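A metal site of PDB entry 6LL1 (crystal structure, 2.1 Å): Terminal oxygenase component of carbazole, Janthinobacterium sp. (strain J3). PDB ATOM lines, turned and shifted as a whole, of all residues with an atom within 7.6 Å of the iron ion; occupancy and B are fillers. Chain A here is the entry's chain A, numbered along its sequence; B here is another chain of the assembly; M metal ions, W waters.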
ATOM      1  N   ASN A 177      -0.067 -29.242  -7.818  1.00  0.00           N
ATOM      2  CA  ASN A 177       0.566 -29.744  -6.629  1.00  0.00           C
ATOM      3  C   ASN A 177       0.691 -28.663  -5.543  1.00  0.00           C
ATOM      4  O   ASN A 177       0.403 -28.882  -4.354  1.00  0.00           O
ATOM      5  CB  ASN A 177       1.944 -30.204  -6.956  1.00  0.00           C
ATOM      6  CG  ASN A 177       2.653 -30.668  -5.751  1.00  0.00           C
ATOM      7  OD1 ASN A 177       2.274 -31.713  -5.158  1.00  0.00           O
ATOM      8  ND2 ASN A 177       3.620 -29.857  -5.290  1.00  0.00           N
ATOM      9  N   GLY A 178       1.139 -27.499  -5.940  1.00  0.00           N
ATOM     10  CA  GLY A 178       1.216 -26.420  -5.022  1.00  0.00           C
ATOM     11  C   GLY A 178      -0.082 -25.987  -4.401  1.00  0.00           C
ATOM     12  O   GLY A 178      -0.096 -25.624  -3.236  1.00  0.00           O
ATOM     13  N   PHE A 179      -1.163 -25.976  -5.172  1.00  0.00           N
ATOM     14  CA  PHE A 179      -2.436 -25.406  -4.656  1.00  0.00           C
ATOM     15  C   PHE A 179      -3.290 -26.506  -4.013  1.00  0.00           C
ATOM     16  O   PHE A 179      -4.374 -26.234  -3.533  1.00  0.00           O
ATOM     17  CB  PHE A 179      -3.182 -24.670  -5.793  1.00  0.00           C
ATOM     18  CG  PHE A 179      -4.380 -23.877  -5.346  1.00  0.00           C
ATOM     19  CD1 PHE A 179      -4.285 -22.955  -4.327  1.00  0.00           C
ATOM     20  CD2 PHE A 179      -5.607 -24.012  -6.023  1.00  0.00           C
ATOM     21  CE1 PHE A 179      -5.387 -22.224  -3.923  1.00  0.00           C
ATOM     22  CE2 PHE A 179      -6.727 -23.244  -5.644  1.00  0.00           C
ATOM     23  CZ  PHE A 179      -6.611 -22.362  -4.587  1.00  0.00           C
ATOM     24  N   ASP A 180      -2.772 -27.734  -3.936  1.00  0.00           N
ATOM     25  CA  ASP A 180      -3.521 -28.936  -3.516  1.00  0.00           C
ATOM     26  C   ASP A 180      -3.622 -29.034  -2.007  1.00  0.00           C
ATOM     27  O   ASP A 180      -2.618 -29.264  -1.354  1.00  0.00           O
ATOM     28  CB  ASP A 180      -2.794 -30.167  -4.072  1.00  0.00           C
ATOM     29  CG  ASP A 180      -3.602 -31.453  -3.950  1.00  0.00           C
ATOM     30  OD1 ASP A 180      -4.389 -31.598  -2.961  1.00  0.00           O
ATOM     31  OD2 ASP A 180      -3.437 -32.311  -4.845  1.00  0.00           O
ATOM     32  N   HIS A 183      -2.046 -32.246  -0.369  1.00  0.00           N
ATOM     33  CA  HIS A 183      -0.768 -32.735  -0.793  1.00  0.00           C
ATOM     34  C   HIS A 183       0.182 -32.593   0.328  1.00  0.00           C
ATOM     35  O   HIS A 183       1.275 -33.128   0.269  1.00  0.00           O
ATOM     36  CB  HIS A 183      -0.244 -31.975  -2.050  1.00  0.00           C
ATOM     37  CG  HIS A 183       0.622 -30.798  -1.746  1.00  0.00           C
ATOM     38  ND1 HIS A 183       0.110 -29.538  -1.484  1.00  0.00           N
ATOM     39  CD2 HIS A 183       1.975 -30.688  -1.659  1.00  0.00           C
ATOM     40  CE1 HIS A 183       1.116 -28.705  -1.242  1.00  0.00           C
ATOM     41  NE2 HIS A 183       2.258 -29.375  -1.341  1.00  0.00           N
ATOM     42  N   ILE A 184      -0.202 -31.830   1.359  1.00  0.00           N
ATOM     43  CA  ILE A 184       0.709 -31.598   2.445  1.00  0.00           C
ATOM     44  C   ILE A 184       1.098 -32.855   3.214  1.00  0.00           C
ATOM     45  O   ILE A 184       2.051 -32.830   3.958  1.00  0.00           O
ATOM     46  CB  ILE A 184       0.174 -30.540   3.440  1.00  0.00           C
ATOM     47  CG1 ILE A 184      -1.177 -30.955   3.993  1.00  0.00           C
ATOM     48  CG2 ILE A 184       0.131 -29.176   2.748  1.00  0.00           C
ATOM     49  CD1 ILE A 184      -1.502 -30.274   5.283  1.00  0.00           C
ATOM     50  N   ILE A 186       2.726 -35.160   1.956  1.00  0.00           N
ATOM     51  CA  ILE A 186       4.072 -35.503   1.522  1.00  0.00           C
ATOM     52  C   ILE A 186       5.086 -34.782   2.326  1.00  0.00           C
ATOM     53  O   ILE A 186       6.256 -35.118   2.252  1.00  0.00           O
ATOM     54  CB  ILE A 186       4.331 -35.224  -0.008  1.00  0.00           C
ATOM     55  CG1 ILE A 186       4.635 -33.728  -0.336  1.00  0.00           C
ATOM     56  CG2 ILE A 186       3.174 -35.743  -0.842  1.00  0.00           C
ATOM     57  CD1 ILE A 186       4.646 -33.415  -1.843  1.00  0.00           C
ATOM     58  N   HIS A 187       4.650 -33.751   3.042  1.00  0.00           N
ATOM     59  CA  HIS A 187       5.562 -32.895   3.833  1.00  0.00           C
ATOM     60  C   HIS A 187       5.663 -33.286   5.325  1.00  0.00           C
ATOM     61  O   HIS A 187       6.365 -32.628   6.082  1.00  0.00           O
ATOM     62  CB  HIS A 187       5.108 -31.429   3.708  1.00  0.00           C
ATOM     63  CG  HIS A 187       5.344 -30.843   2.355  1.00  0.00           C
ATOM     64  ND1 HIS A 187       6.602 -30.801   1.766  1.00  0.00           N
ATOM     65  CD2 HIS A 187       4.491 -30.270   1.470  1.00  0.00           C
ATOM     66  CE1 HIS A 187       6.501 -30.214   0.577  1.00  0.00           C
ATOM     67  NE2 HIS A 187       5.246 -29.857   0.387  1.00  0.00           N
ATOM     68  N   LEU A 270       1.621 -19.077  -6.928  1.00  0.00           N
ATOM     69  CA  LEU A 270       1.008 -19.500  -5.663  1.00  0.00           C
ATOM     70  C   LEU A 270       1.528 -18.541  -4.621  1.00  0.00           C
ATOM     71  O   LEU A 270       2.727 -18.259  -4.613  1.00  0.00           O
ATOM     72  CB  LEU A 270       1.471 -20.917  -5.264  1.00  0.00           C
ATOM     73  CG  LEU A 270       0.923 -21.458  -3.934  1.00  0.00           C
ATOM     74  CD1 LEU A 270      -0.471 -22.025  -4.176  1.00  0.00           C
ATOM     75  CD2 LEU A 270       1.839 -22.532  -3.367  1.00  0.00           C
ATOM     76  N   PHE A 275       4.440 -18.112   5.597  1.00  0.00           N
ATOM     77  CA  PHE A 275       5.266 -19.319   5.288  1.00  0.00           C
ATOM     78  C   PHE A 275       6.652 -18.909   4.799  1.00  0.00           C
ATOM     79  O   PHE A 275       6.742 -17.896   4.120  1.00  0.00           O
ATOM     80  CB  PHE A 275       4.614 -20.195   4.193  1.00  0.00           C
ATOM     81  CG  PHE A 275       5.094 -21.634   4.210  1.00  0.00           C
ATOM     82  CD1 PHE A 275       4.481 -22.566   5.014  1.00  0.00           C
ATOM     83  CD2 PHE A 275       6.173 -22.036   3.451  1.00  0.00           C
ATOM     84  CE1 PHE A 275       4.934 -23.886   5.045  1.00  0.00           C
ATOM     85  CE2 PHE A 275       6.643 -23.348   3.493  1.00  0.00           C
ATOM     86  CZ  PHE A 275       6.022 -24.264   4.273  1.00  0.00           C
ATOM     87  N   GLU A 284       5.582 -18.405  -5.367  1.00  0.00           N
ATOM     88  CA  GLU A 284       6.290 -19.242  -6.295  1.00  0.00           C
ATOM     89  C   GLU A 284       5.520 -19.414  -7.591  1.00  0.00           C
ATOM     90  O   GLU A 284       4.307 -19.633  -7.603  1.00  0.00           O
ATOM     91  CB  GLU A 284       6.648 -20.596  -5.682  1.00  0.00           C
ATOM     92  CG  GLU A 284       5.501 -21.390  -5.083  1.00  0.00           C
ATOM     93  CD  GLU A 284       5.997 -22.758  -4.584  1.00  0.00           C
ATOM     94  OE1 GLU A 284       7.053 -22.843  -3.891  1.00  0.00           O
ATOM     95  OE2 GLU A 284       5.381 -23.758  -4.977  1.00  0.00           O
ATOM     96  N   TYR A 286       5.433 -21.202 -11.522  1.00  0.00           N
ATOM     97  CA  TYR A 286       5.687 -22.391 -12.271  1.00  0.00           C
ATOM     98  C   TYR A 286       5.551 -21.991 -13.758  1.00  0.00           C
ATOM     99  O   TYR A 286       4.442 -22.040 -14.361  1.00  0.00           O
ATOM    100  CB  TYR A 286       4.710 -23.487 -11.870  1.00  0.00           C
ATOM    101  CG  TYR A 286       4.369 -23.519 -10.386  1.00  0.00           C
ATOM    102  CD1 TYR A 286       5.203 -24.130  -9.473  1.00  0.00           C
ATOM    103  CD2 TYR A 286       3.179 -22.933  -9.936  1.00  0.00           C
ATOM    104  CE1 TYR A 286       4.861 -24.167  -8.142  1.00  0.00           C
ATOM    105  CE2 TYR A 286       2.833 -22.943  -8.589  1.00  0.00           C
ATOM    106  CZ  TYR A 286       3.676 -23.559  -7.696  1.00  0.00           C
ATOM    107  OH  TYR A 286       3.291 -23.562  -6.381  1.00  0.00           O
ATOM    108  N   TYR A 296      10.820 -23.398 -11.803  1.00  0.00           N
ATOM    109  CA  TYR A 296      10.274 -23.320 -10.488  1.00  0.00           C
ATOM    110  C   TYR A 296      10.957 -22.100  -9.807  1.00  0.00           C
ATOM    111  O   TYR A 296      12.088 -22.217  -9.325  1.00  0.00           O
ATOM    112  CB  TYR A 296      10.553 -24.630  -9.757  1.00  0.00           C
ATOM    113  CG  TYR A 296      10.026 -24.704  -8.362  1.00  0.00           C
ATOM    114  CD1 TYR A 296       8.883 -24.039  -7.984  1.00  0.00           C
ATOM    115  CD2 TYR A 296      10.670 -25.480  -7.407  1.00  0.00           C
ATOM    116  CE1 TYR A 296       8.406 -24.131  -6.729  1.00  0.00           C
ATOM    117  CE2 TYR A 296      10.182 -25.581  -6.113  1.00  0.00           C
ATOM    118  CZ  TYR A 296       9.059 -24.898  -5.768  1.00  0.00           C
ATOM    119  OH  TYR A 296       8.602 -24.946  -4.479  1.00  0.00           O
ATOM    120  N   PHE A 329      12.021 -28.246   2.470  1.00  0.00           N
ATOM    121  CA  PHE A 329      10.596 -28.528   2.372  1.00  0.00           C
ATOM    122  C   PHE A 329      10.100 -28.723   0.918  1.00  0.00           C
ATOM    123  O   PHE A 329       9.391 -29.680   0.647  1.00  0.00           O
ATOM    124  CB  PHE A 329       9.861 -27.388   3.053  1.00  0.00           C
ATOM    125  CG  PHE A 329       8.393 -27.596   3.206  1.00  0.00           C
ATOM    126  CD1 PHE A 329       7.877 -28.187   4.356  1.00  0.00           C
ATOM    127  CD2 PHE A 329       7.516 -27.107   2.241  1.00  0.00           C
ATOM    128  CE1 PHE A 329       6.503 -28.316   4.521  1.00  0.00           C
ATOM    129  CE2 PHE A 329       6.164 -27.220   2.387  1.00  0.00           C
ATOM    130  CZ  PHE A 329       5.649 -27.821   3.535  1.00  0.00           C
ATOM    131  N   ASN A 330      10.480 -27.864  -0.022  1.00  0.00           N
ATOM    132  CA  ASN A 330       9.937 -27.991  -1.416  1.00  0.00           C
ATOM    133  C   ASN A 330      10.504 -29.083  -2.307  1.00  0.00           C
ATOM    134  O   ASN A 330       9.864 -29.422  -3.327  1.00  0.00           O
ATOM    135  CB  ASN A 330       9.967 -26.659  -2.145  1.00  0.00           C
ATOM    136  CG  ASN A 330       9.054 -25.644  -1.499  1.00  0.00           C
ATOM    137  OD1 ASN A 330       9.490 -24.630  -1.085  1.00  0.00           O
ATOM    138  ND2 ASN A 330       7.796 -25.986  -1.343  1.00  0.00           N
ATOM    139  N   ASP A 332      10.339 -32.127  -1.815  1.00  0.00           N
ATOM    140  CA  ASP A 332       9.283 -33.132  -2.021  1.00  0.00           C
ATOM    141  C   ASP A 332       8.284 -32.760  -3.104  1.00  0.00           C
ATOM    142  O   ASP A 332       7.758 -33.673  -3.777  1.00  0.00           O
ATOM    143  CB  ASP A 332       8.514 -33.444  -0.758  1.00  0.00           C
ATOM    144  CG  ASP A 332       9.345 -34.235   0.227  1.00  0.00           C
ATOM    145  OD1 ASP A 332      10.077 -35.162  -0.184  1.00  0.00           O
ATOM    146  OD2 ASP A 332       9.323 -33.886   1.407  1.00  0.00           O
ATOM    147  N   ASP A 333       8.005 -31.468  -3.232  1.00  0.00           N
ATOM    148  CA  ASP A 333       7.094 -30.988  -4.288  1.00  0.00           C
ATOM    149  C   ASP A 333       7.642 -31.354  -5.648  1.00  0.00           C
ATOM    150  O   ASP A 333       6.876 -31.757  -6.530  1.00  0.00           O
ATOM    151  CB  ASP A 333       6.821 -29.473  -4.184  1.00  0.00           C
ATOM    152  CG  ASP A 333       6.093 -29.098  -2.910  1.00  0.00           C
ATOM    153  OD1 ASP A 333       4.924 -29.479  -2.761  1.00  0.00           O
ATOM    154  OD2 ASP A 333       6.662 -28.449  -2.032  1.00  0.00           O
ATOM    155  N   ILE A 334       8.975 -31.292  -5.794  1.00  0.00           N
ATOM    156  CA  ILE A 334       9.596 -31.523  -7.070  1.00  0.00           C
ATOM    157  C   ILE A 334       9.388 -32.950  -7.513  1.00  0.00           C
ATOM    158  O   ILE A 334       8.948 -33.174  -8.627  1.00  0.00           O
ATOM    159  CB  ILE A 334      11.108 -31.203  -7.043  1.00  0.00           C
ATOM    160  CG1 ILE A 334      11.306 -29.688  -6.970  1.00  0.00           C
ATOM    161  CG2 ILE A 334      11.834 -31.798  -8.254  1.00  0.00           C
ATOM    162  CD1 ILE A 334      12.677 -29.296  -6.421  1.00  0.00           C
ATOM    163  N   ALA A 336       7.121 -35.083  -6.404  1.00  0.00           N
ATOM    164  CA  ALA A 336       5.629 -35.283  -6.636  1.00  0.00           C
ATOM    165  C   ALA A 336       5.155 -34.887  -8.066  1.00  0.00           C
ATOM    166  O   ALA A 336       4.527 -35.659  -8.773  1.00  0.00           O
ATOM    167  CB  ALA A 336       4.801 -34.528  -5.584  1.00  0.00           C
ATOM    168  N   ARG A 337       5.525 -33.675  -8.495  1.00  0.00           N
ATOM    169  CA  ARG A 337       5.242 -33.207  -9.883  1.00  0.00           C
ATOM    170  C   ARG A 337       5.697 -34.187 -10.904  1.00  0.00           C
ATOM    171  O   ARG A 337       4.955 -34.575 -11.804  1.00  0.00           O
ATOM    172  CB  ARG A 337       6.037 -31.951 -10.183  1.00  0.00           C
ATOM    173  CG  ARG A 337       5.554 -30.783  -9.391  1.00  0.00           C
ATOM    174  CD  ARG A 337       6.497 -29.643  -9.589  1.00  0.00           C
ATOM    175  NE  ARG A 337       6.399 -28.853  -8.404  1.00  0.00           N
ATOM    176  CZ  ARG A 337       7.157 -27.812  -8.099  1.00  0.00           C
ATOM    177  NH1 ARG A 337       8.057 -27.370  -8.954  1.00  0.00           N
ATOM    178  NH2 ARG A 337       6.952 -27.191  -6.943  1.00  0.00           N
ATOM    179  N   TYR B  92       1.097 -39.773  -1.621  1.00  0.00           N
ATOM    180  CA  TYR B  92       0.843 -38.407  -2.149  1.00  0.00           C
ATOM    181  C   TYR B  92      -0.277 -37.740  -1.338  1.00  0.00           C
ATOM    182  O   TYR B  92      -0.027 -36.762  -0.687  1.00  0.00           O
ATOM    183  CB  TYR B  92       0.478 -38.438  -3.643  1.00  0.00           C
ATOM    184  CG  TYR B  92       0.598 -37.130  -4.398  1.00  0.00           C
ATOM    185  CD1 TYR B  92       0.938 -35.912  -3.757  1.00  0.00           C
ATOM    186  CD2 TYR B  92       0.377 -37.098  -5.763  1.00  0.00           C
ATOM    187  CE1 TYR B  92       1.034 -34.722  -4.448  1.00  0.00           C
ATOM    188  CE2 TYR B  92       0.490 -35.914  -6.469  1.00  0.00           C
ATOM    189  CZ  TYR B  92       0.799 -34.720  -5.816  1.00  0.00           C
ATOM    190  OH  TYR B  92       0.926 -33.551  -6.506  1.00  0.00           O
HETATM  191 FE    FE M   1       4.109 -28.722  -1.106  1.00  0.00          FE
HETATM  192  O   HOH W   1       4.078 -26.862  -0.715  1.00  0.00           O
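O of Asp 333 lies close to NE of Arg 337 (3.5 Å). O of Asp 180 sits at hydrogen-bond distance from ND1 of His 183 (2.7 Å). A ring nitrogen (ND1) of His 187 lies close to the backbone carbonyl oxygen (O) of Phe 329 (3.2 Å). ND1 of His 183 sits at hydrogen-bond distance from O of Asn 177 (3.0 Å). OD1 of Asp 333 lies close to ND2 of Asn 177 (2.9 Å). The side-chain amide nitrogen (ND2) of Asn 330 sits at hydrogen-bond distance from the side-chain carboxylate (OD2) of Asp 333 (2.8 Å).
Of the 21 residues printed, 3 come within 4 Å of the iron ion.
The iron ion is bound by water W1 (1.9 Å), NE2 of His 183 (2.0 Å), OD1 of Asp 333 (2.0 Å) and NE2 of His 187 (2.2 Å). The iron ion has four donor atoms within binding distance. Slightly farther from the iron ion lies the side-chain carboxylate (OD2) of Asp 333 (2.7 Å).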
